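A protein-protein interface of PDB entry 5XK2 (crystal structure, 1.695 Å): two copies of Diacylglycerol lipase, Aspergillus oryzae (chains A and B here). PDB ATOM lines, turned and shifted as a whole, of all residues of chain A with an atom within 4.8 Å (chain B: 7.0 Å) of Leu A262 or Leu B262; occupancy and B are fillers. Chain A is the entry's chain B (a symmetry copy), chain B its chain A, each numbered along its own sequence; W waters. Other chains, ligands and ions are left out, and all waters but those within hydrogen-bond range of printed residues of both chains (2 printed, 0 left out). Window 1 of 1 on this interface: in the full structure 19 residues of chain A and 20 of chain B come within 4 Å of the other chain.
Hydrophobic or aromatic side chains of chain B within 4 Å of the printed part of chain A: Val B98, Leu B211, Leu B259, Pro B260, Leu B262, Leu B263 and Phe B265.
Of the 10 printed residues of chain A, 8 touch a printed residue of chain B.
Hydrophobic or aromatic side chains of chain A that line the printed part of chain B: Ile A94, Val A98, Leu A211, Pro A260, Leu A262, Leu A263 and Phe A265.
Leu A211 touches Leu B262, and with the chains exchanged Leu A262 touches Leu B211.
Leu A211 touches Leu B263, and with the chains exchanged Leu A263 touches Leu B211.
Pro B260 touches its own counterpart, Pro A260.
Pro A260 touches Asp B261, and with the chains exchanged Asp A261 touches Pro B260.
10 positions are printed for both chains.
Of the 19 pairs that touch across the chains among the printed residues, 14 have their exchanged pair printed and touching as well.
Water W2 lies within hydrogen-bond range of the backbone carbonyl oxygen (O) of Val A98, the backbone carbonyl oxygen (O) of Leu B263, the backbone NH (N) of His B266 and the backbone NH (N) of Phe B265.
Water W1 lies within hydrogen-bond range of the backbone carbonyl oxygen of Val B98 (2.6 Å), the backbone carbonyl oxygen of Leu A263 (2.8 Å) and the backbone NH of Phe A265 (3.4 Å).
Leu B262 touches just these residues of chain A: Ile A94 (3.96 Å), Val A98 (3.9 Å), Leu A211 (3.9 Å), Pro A260 (2.8 Å) and Leu A262 (3.9 Å).
Printed residues of chain B within 4 Å of Ile A94: Arg B95 and Leu B262.
Printed residues of chain B within 4 Å of Val A98: Leu B262 (3.9 Å) and Phe B265 (3.9 Å).
The nearest printed residue of chain B that does not touch Leu A262 is Pro B207 (4.01 Å).
The nearest printed residue of chain A that does not touch Phe B265 is Leu A262 (5.4 Å).
The backbone carbonyl oxygen (O) of Pro B260 is in hydrogen-bond range of the backbone NH (N) of Leu A262 (2.7 Å).
The backbone carbonyl oxygen of Pro A260 lies within hydrogen-bond range of the backbone NH of Leu B262, 2.8 Å away.
The side-chain hydroxyl of Thr B99 is in hydrogen-bond range of the backbone carbonyl oxygen of Arg B95 (2.6 Å).
The backbone NH (N) of Leu B263 sits at hydrogen-bond distance from the side-chain carboxylate (OD1) of Asp B261 (2.8 Å).
The side-chain carboxylate of Asp A261 lies within hydrogen-bond range of the backbone NH of Leu A263 (2.9 Å).
Among the printed residues, pairs that only touch across the chains: Phe A265 with Thr B99 (3.4 Å), Asp A261 with Pro B260 (3.4 Å), Pro A260 with Asp B261 (3.5 Å), Phe A265 with Arg B95 (3.5 Å), Asp A261 with Leu B259 (3.7 Å), Pro A260 with Pro B260 (3.7 Å), Ile A94 with Arg B95 (3.8 Å), Val A98 with Leu B262 (3.9 Å), Leu A263 with Leu B211 (3.9 Å), Leu A211 with Leu B263 (3.9 Å), Leu A262 with Val B98 (3.9 Å), Leu A211 with Leu B262 (3.9 Å), Val A98 with Phe B265 (3.9 Å), Leu A262 with Leu B262 (3.9 Å), Phe A265 with Val B98 (3.9 Å), Ile A94 with Leu B262 (3.96 Å) and Leu A262 with Leu B211 (3.96 Å).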
ATOM      1  N   ILE A  94      12.778  14.437  26.992  1.00  0.00           N
ATOM      2  CA  ILE A  94      13.869  13.524  26.716  1.00  0.00           C
ATOM      3  C   ILE A  94      14.593  14.019  25.475  1.00  0.00           C
ATOM      4  O   ILE A  94      15.822  13.988  25.423  1.00  0.00           O
ATOM      5  CB  ILE A  94      13.374  12.075  26.526  1.00  0.00           C
ATOM      6  CG1 ILE A  94      12.854  11.515  27.853  1.00  0.00           C
ATOM      7  CG2 ILE A  94      14.496  11.184  26.011  1.00  0.00           C
ATOM      8  CD1 ILE A  94      13.891  11.501  28.966  1.00  0.00           C
ATOM      9  N   VAL A  98      18.702  14.763  25.043  1.00  0.00           N
ATOM     10  CA  VAL A  98      19.621  14.089  24.132  1.00  0.00           C
ATOM     11  C   VAL A  98      19.969  14.801  22.820  1.00  0.00           C
ATOM     12  O   VAL A  98      20.919  14.381  22.156  1.00  0.00           O
ATOM     13  CB  VAL A  98      19.086  12.689  23.740  1.00  0.00           C
ATOM     14  CG1 VAL A  98      18.830  11.841  24.981  1.00  0.00           C
ATOM     15  CG2 VAL A  98      17.816  12.817  22.905  1.00  0.00           C
ATOM     16  N   PRO A 207      15.594   2.512  27.548  1.00  0.00           N
ATOM     17  CA  PRO A 207      16.790   3.123  26.957  1.00  0.00           C
ATOM     18  C   PRO A 207      17.511   4.112  27.876  1.00  0.00           C
ATOM     19  O   PRO A 207      18.713   4.321  27.684  1.00  0.00           O
ATOM     20  CB  PRO A 207      16.239   3.852  25.729  1.00  0.00           C
ATOM     21  CG  PRO A 207      14.836   4.196  26.103  1.00  0.00           C
ATOM     22  CD  PRO A 207      14.355   2.974  26.898  1.00  0.00           C
ATOM     23  N   LEU A 211      22.260   5.766  29.038  1.00  0.00           N
ATOM     24  CA  LEU A 211      22.811   7.082  28.718  1.00  0.00           C
ATOM     25  C   LEU A 211      23.255   7.818  29.978  1.00  0.00           C
ATOM     26  O   LEU A 211      22.649   7.655  31.032  1.00  0.00           O
ATOM     27  CB  LEU A 211      21.779   7.933  27.972  1.00  0.00           C
ATOM     28  CG  LEU A 211      21.365   7.455  26.568  1.00  0.00           C
ATOM     29  CD1 LEU A 211      20.250   8.339  26.048  1.00  0.00           C
ATOM     30  CD2 LEU A 211      22.545   7.478  25.614  1.00  0.00           C
ATOM     31  N   PRO A 260      20.364   2.185  23.003  1.00  0.00           N
ATOM     32  CA  PRO A 260      19.172   2.810  23.590  1.00  0.00           C
ATOM     33  C   PRO A 260      18.044   2.916  22.553  1.00  0.00           C
ATOM     34  O   PRO A 260      18.045   3.834  21.728  1.00  0.00           O
ATOM     35  CB  PRO A 260      19.669   4.184  24.055  1.00  0.00           C
ATOM     36  CG  PRO A 260      20.922   4.433  23.332  1.00  0.00           C
ATOM     37  CD  PRO A 260      21.348   3.199  22.588  1.00  0.00           C
ATOM     38  N   ASP A 261      17.173   1.916  22.515  1.00  0.00           N
ATOM     39  CA  ASP A 261      16.071   1.859  21.551  1.00  0.00           C
ATOM     40  C   ASP A 261      14.966   2.867  21.903  1.00  0.00           C
ATOM     41  O   ASP A 261      14.359   2.792  22.984  1.00  0.00           O
ATOM     42  CB  ASP A 261      15.516   0.427  21.528  1.00  0.00           C
ATOM     43  CG  ASP A 261      14.544   0.166  20.386  1.00  0.00           C
ATOM     44  OD1 ASP A 261      13.904   1.107  19.873  1.00  0.00           O
ATOM     45  OD2 ASP A 261      14.395  -1.021  20.014  1.00  0.00           O
ATOM     46  N   LEU A 262      14.694   3.802  20.989  1.00  0.00           N
ATOM     47  CA  LEU A 262      13.656   4.815  21.209  1.00  0.00           C
ATOM     48  C   LEU A 262      12.301   4.185  21.448  1.00  0.00           C
ATOM     49  O   LEU A 262      11.502   4.683  22.249  1.00  0.00           O
ATOM     50  CB  LEU A 262      13.575   5.781  20.014  1.00  0.00           C
ATOM     51  CG  LEU A 262      12.405   6.770  19.970  1.00  0.00           C
ATOM     52  CD1 LEU A 262      12.472   7.713  21.149  1.00  0.00           C
ATOM     53  CD2 LEU A 262      12.465   7.558  18.678  1.00  0.00           C
ATOM     54  N   LEU A 263      12.035   3.080  20.763  1.00  0.00           N
ATOM     55  CA  LEU A 263      10.719   2.466  20.881  1.00  0.00           C
ATOM     56  C   LEU A 263      10.584   1.663  22.175  1.00  0.00           C
ATOM     57  O   LEU A 263       9.493   1.209  22.535  1.00  0.00           O
ATOM     58  CB  LEU A 263      10.438   1.588  19.661  1.00  0.00           C
ATOM     59  CG  LEU A 263       9.002   1.068  19.561  1.00  0.00           C
ATOM     60  CD1 LEU A 263       7.969   2.187  19.513  1.00  0.00           C
ATOM     61  CD2 LEU A 263       8.882   0.169  18.350  1.00  0.00           C
ATOM     62  N   ALA A 264      11.682   1.535  22.909  1.00  0.00           N
ATOM     63  CA  ALA A 264      11.626   0.858  24.201  1.00  0.00           C
ATOM     64  C   ALA A 264      11.245   1.833  25.302  1.00  0.00           C
ATOM     65  O   ALA A 264      11.262   1.481  26.481  1.00  0.00           O
ATOM     66  CB  ALA A 264      12.963   0.195  24.512  1.00  0.00           C
ATOM     67  N   PHE A 265      10.908   3.067  24.929  1.00  0.00           N
ATOM     68  CA  PHE A 265      10.628   4.079  25.939  1.00  0.00           C
ATOM     69  C   PHE A 265       9.476   3.721  26.870  1.00  0.00           C
ATOM     70  O   PHE A 265       9.455   4.157  28.025  1.00  0.00           O
ATOM     71  CB  PHE A 265      10.357   5.445  25.302  1.00  0.00           C
ATOM     72  CG  PHE A 265      10.469   6.566  26.288  1.00  0.00           C
ATOM     73  CD1 PHE A 265      11.713   7.053  26.656  1.00  0.00           C
ATOM     74  CD2 PHE A 265       9.339   7.078  26.906  1.00  0.00           C
ATOM     75  CE1 PHE A 265      11.835   8.068  27.604  1.00  0.00           C
ATOM     76  CE2 PHE A 265       9.446   8.090  27.853  1.00  0.00           C
ATOM     77  CZ  PHE A 265      10.694   8.585  28.201  1.00  0.00           C
ATOM     78  N   ILE B  94       8.035  13.644  21.398  1.00  0.00           N
ATOM     79  CA  ILE B  94       8.355  12.343  20.829  1.00  0.00           C
ATOM     80  C   ILE B  94       8.064  11.255  21.845  1.00  0.00           C
ATOM     81  O   ILE B  94       7.559  10.187  21.495  1.00  0.00           O
ATOM     82  CB  ILE B  94       9.829  12.258  20.398  1.00  0.00           C
ATOM     83  CG1 ILE B  94      10.120  13.282  19.299  1.00  0.00           C
ATOM     84  CG2 ILE B  94      10.162  10.851  19.914  1.00  0.00           C
ATOM     85  CD1 ILE B  94       9.408  12.995  17.979  1.00  0.00           C
ATOM     86  N   ARG B  95       8.358  11.528  23.116  1.00  0.00           N
ATOM     87  CA  ARG B  95       8.108  10.519  24.137  1.00  0.00           C
ATOM     88  C   ARG B  95       6.612  10.192  24.222  1.00  0.00           C
ATOM     89  O   ARG B  95       6.248   9.031  24.342  1.00  0.00           O
ATOM     90  CB  ARG B  95       8.674  10.950  25.506  1.00  0.00           C
ATOM     91  CG  ARG B  95       7.948  12.086  26.212  1.00  0.00           C
ATOM     92  CD  ARG B  95       8.587  12.390  27.572  1.00  0.00           C
ATOM     93  NE  ARG B  95       8.291  11.364  28.574  1.00  0.00           N
ATOM     94  CZ  ARG B  95       8.897  11.261  29.755  1.00  0.00           C
ATOM     95  NH1 ARG B  95       9.840  12.125  30.109  1.00  0.00           N
ATOM     96  NH2 ARG B  95       8.552  10.292  30.593  1.00  0.00           N
ATOM     97  N   TRP B  97       4.467  10.373  21.815  1.00  0.00           N
ATOM     98  CA  TRP B  97       4.128   9.674  20.584  1.00  0.00           C
ATOM     99  C   TRP B  97       4.454   8.177  20.685  1.00  0.00           C
ATOM    100  O   TRP B  97       3.688   7.331  20.225  1.00  0.00           O
ATOM    101  CB  TRP B  97       4.885  10.315  19.417  1.00  0.00           C
ATOM    102  CG  TRP B  97       4.632   9.696  18.106  1.00  0.00           C
ATOM    103  CD1 TRP B  97       3.424   9.490  17.521  1.00  0.00           C
ATOM    104  CD2 TRP B  97       5.619   9.219  17.176  1.00  0.00           C
ATOM    105  NE1 TRP B  97       3.590   8.902  16.291  1.00  0.00           N
ATOM    106  CE2 TRP B  97       4.928   8.725  16.056  1.00  0.00           C
ATOM    107  CE3 TRP B  97       7.019   9.157  17.188  1.00  0.00           C
ATOM    108  CZ2 TRP B  97       5.582   8.167  14.956  1.00  0.00           C
ATOM    109  CZ3 TRP B  97       7.669   8.603  16.092  1.00  0.00           C
ATOM    110  CH2 TRP B  97       6.951   8.117  14.994  1.00  0.00           C
ATOM    111  N   VAL B  98       5.607   7.855  21.271  1.00  0.00           N
ATOM    112  CA  VAL B  98       6.035   6.459  21.320  1.00  0.00           C
ATOM    113  C   VAL B  98       5.700   5.691  22.600  1.00  0.00           C
ATOM    114  O   VAL B  98       5.808   4.464  22.603  1.00  0.00           O
ATOM    115  CB  VAL B  98       7.576   6.332  21.100  1.00  0.00           C
ATOM    116  CG1 VAL B  98       7.988   6.967  19.778  1.00  0.00           C
ATOM    117  CG2 VAL B  98       8.354   6.940  22.261  1.00  0.00           C
ATOM    118  N   THR B  99       5.270   6.372  23.665  1.00  0.00           N
ATOM    119  CA  THR B  99       5.201   5.717  24.983  1.00  0.00           C
ATOM    120  C   THR B  99       4.232   4.523  25.030  1.00  0.00           C
ATOM    121  O   THR B  99       4.518   3.528  25.699  1.00  0.00           O
ATOM    122  CB  THR B  99       4.854   6.734  26.086  1.00  0.00           C
ATOM    123  OG1 THR B  99       6.023   7.509  26.377  1.00  0.00           O
ATOM    124  CG2 THR B  99       4.426   6.041  27.381  1.00  0.00           C
ATOM    125  N   PRO B 207      16.251   8.486  14.116  1.00  0.00           N
ATOM    126  CA  PRO B 207      15.390   7.357  14.503  1.00  0.00           C
ATOM    127  C   PRO B 207      13.924   7.470  14.062  1.00  0.00           C
ATOM    128  O   PRO B 207      13.228   6.450  13.956  1.00  0.00           O
ATOM    129  CB  PRO B 207      15.475   7.356  16.033  1.00  0.00           C
ATOM    130  CG  PRO B 207      15.766   8.778  16.400  1.00  0.00           C
ATOM    131  CD  PRO B 207      16.685   9.289  15.279  1.00  0.00           C
ATOM    132  N   VAL B 208      13.444   8.692  13.852  1.00  0.00           N
ATOM    133  CA  VAL B 208      12.009   8.886  13.660  1.00  0.00           C
ATOM    134  C   VAL B 208      11.465   8.227  12.379  1.00  0.00           C
ATOM    135  O   VAL B 208      10.407   7.607  12.441  1.00  0.00           O
ATOM    136  CB  VAL B 208      11.662  10.393  13.738  1.00  0.00           C
ATOM    137  CG1 VAL B 208      10.171  10.632  13.454  1.00  0.00           C
ATOM    138  CG2 VAL B 208      12.008  10.915  15.163  1.00  0.00           C
ATOM    139  N   LEU B 211      10.004   4.585  12.482  1.00  0.00           N
ATOM    140  CA  LEU B 211       8.763   4.305  13.212  1.00  0.00           C
ATOM    141  C   LEU B 211       7.554   4.783  12.428  1.00  0.00           C
ATOM    142  O   LEU B 211       7.639   5.756  11.685  1.00  0.00           O
ATOM    143  CB  LEU B 211       8.771   4.983  14.580  1.00  0.00           C
ATOM    144  CG  LEU B 211       9.845   4.492  15.549  1.00  0.00           C
ATOM    145  CD1 LEU B 211       9.773   5.328  16.807  1.00  0.00           C
ATOM    146  CD2 LEU B 211       9.654   3.010  15.847  1.00  0.00           C
ATOM    147  N   LEU B 259      17.690  -0.469  14.223  1.00  0.00           N
ATOM    148  CA  LEU B 259      16.939   0.037  15.373  1.00  0.00           C
ATOM    149  C   LEU B 259      16.862   1.577  15.396  1.00  0.00           C
ATOM    150  O   LEU B 259      17.750   2.246  14.878  1.00  0.00           O
ATOM    151  CB  LEU B 259      17.583  -0.451  16.679  1.00  0.00           C
ATOM    152  CG  LEU B 259      17.441  -1.922  17.079  1.00  0.00           C
ATOM    153  CD1 LEU B 259      17.947  -2.110  18.501  1.00  0.00           C
ATOM    154  CD2 LEU B 259      16.003  -2.392  16.966  1.00  0.00           C
ATOM    155  N   PRO B 260      15.799   2.140  15.995  1.00  0.00           N
ATOM    156  CA  PRO B 260      15.698   3.585  16.252  1.00  0.00           C
ATOM    157  C   PRO B 260      16.505   3.997  17.481  1.00  0.00           C
ATOM    158  O   PRO B 260      16.045   3.797  18.598  1.00  0.00           O
ATOM    159  CB  PRO B 260      14.196   3.831  16.442  1.00  0.00           C
ATOM    160  CG  PRO B 260      13.613   2.503  16.792  1.00  0.00           C
ATOM    161  CD  PRO B 260      14.548   1.423  16.310  1.00  0.00           C
ATOM    162  N   ASP B 261      17.733   4.452  17.274  1.00  0.00           N
ATOM    163  CA  ASP B 261      18.619   4.850  18.371  1.00  0.00           C
ATOM    164  C   ASP B 261      18.205   6.196  18.978  1.00  0.00           C
ATOM    165  O   ASP B 261      18.198   7.222  18.294  1.00  0.00           O
ATOM    166  CB  ASP B 261      20.051   4.915  17.813  1.00  0.00           C
ATOM    167  CG  ASP B 261      21.110   5.262  18.860  1.00  0.00           C
ATOM    168  OD1 ASP B 261      20.793   5.567  20.031  1.00  0.00           O
ATOM    169  OD2 ASP B 261      22.300   5.249  18.468  1.00  0.00           O
ATOM    170  N   LEU B 262      17.856   6.190  20.262  1.00  0.00           N
ATOM    171  CA  LEU B 262      17.473   7.414  20.953  1.00  0.00           C
ATOM    172  C   LEU B 262      18.573   8.476  20.874  1.00  0.00           C
ATOM    173  O   LEU B 262      18.285   9.672  20.716  1.00  0.00           O
ATOM    174  CB  LEU B 262      17.138   7.104  22.420  1.00  0.00           C
ATOM    175  CG  LEU B 262      16.906   8.304  23.344  1.00  0.00           C
ATOM    176  CD1 LEU B 262      15.720   9.123  22.863  1.00  0.00           C
ATOM    177  CD2 LEU B 262      16.630   7.788  24.738  1.00  0.00           C
ATOM    178  N   LEU B 263      19.827   8.051  20.958  1.00  0.00           N
ATOM    179  CA  LEU B 263      20.921   9.021  20.967  1.00  0.00           C
ATOM    180  C   LEU B 263      21.200   9.573  19.575  1.00  0.00           C
ATOM    181  O   LEU B 263      21.944  10.537  19.427  1.00  0.00           O
ATOM    182  CB  LEU B 263      22.197   8.409  21.558  1.00  0.00           C
ATOM    183  CG  LEU B 263      23.256   9.446  21.955  1.00  0.00           C
ATOM    184  CD1 LEU B 263      22.722  10.479  22.945  1.00  0.00           C
ATOM    185  CD2 LEU B 263      24.479   8.743  22.516  1.00  0.00           C
ATOM    186  N   ALA B 264      20.566   8.994  18.555  1.00  0.00           N
ATOM    187  CA  ALA B 264      20.693   9.536  17.196  1.00  0.00           C
ATOM    188  C   ALA B 264      19.698  10.675  16.957  1.00  0.00           C
ATOM    189  O   ALA B 264      19.578  11.183  15.842  1.00  0.00           O
ATOM    190  CB  ALA B 264      20.508   8.444  16.166  1.00  0.00           C
ATOM    191  N   PHE B 265      18.974  11.086  17.996  1.00  0.00           N
ATOM    192  CA  PHE B 265      17.943  12.083  17.798  1.00  0.00           C
ATOM    193  C   PHE B 265      18.474  13.407  17.229  1.00  0.00           C
ATOM    194  O   PHE B 265      17.760  14.097  16.512  1.00  0.00           O
ATOM    195  CB  PHE B 265      17.179  12.351  19.096  1.00  0.00           C
ATOM    196  CG  PHE B 265      15.903  13.069  18.859  1.00  0.00           C
ATOM    197  CD1 PHE B 265      14.800  12.390  18.388  1.00  0.00           C
ATOM    198  CD2 PHE B 265      15.829  14.446  19.021  1.00  0.00           C
ATOM    199  CE1 PHE B 265      13.629  13.056  18.126  1.00  0.00           C
ATOM    200  CE2 PHE B 265      14.650  15.125  18.762  1.00  0.00           C
ATOM    201  CZ  PHE B 265      13.552  14.429  18.313  1.00  0.00           C
ATOM    202  N   HIS B 266      19.732  13.739  17.501  1.00  0.00           N
ATOM    203  CA  HIS B 266      20.326  14.950  16.931  1.00  0.00           C
ATOM    204  C   HIS B 266      20.118  15.006  15.409  1.00  0.00           C
ATOM    205  O   HIS B 266      19.899  16.074  14.849  1.00  0.00           O
ATOM    206  CB  HIS B 266      21.823  15.016  17.263  1.00  0.00           C
ATOM    207  CG  HIS B 266      22.630  13.929  16.627  1.00  0.00           C
ATOM    208  ND1 HIS B 266      23.298  14.097  15.430  1.00  0.00           N
ATOM    209  CD2 HIS B 266      22.834  12.637  16.993  1.00  0.00           C
ATOM    210  CE1 HIS B 266      23.904  12.966  15.102  1.00  0.00           C
ATOM    211  NE2 HIS B 266      23.641  12.067  16.033  1.00  0.00           N
HETATM  212  O   HOH W   1       7.710   2.991  23.672  1.00  0.00           O
HETATM  213  O   HOH W   2      20.959  12.982  19.950  1.00  0.00           O
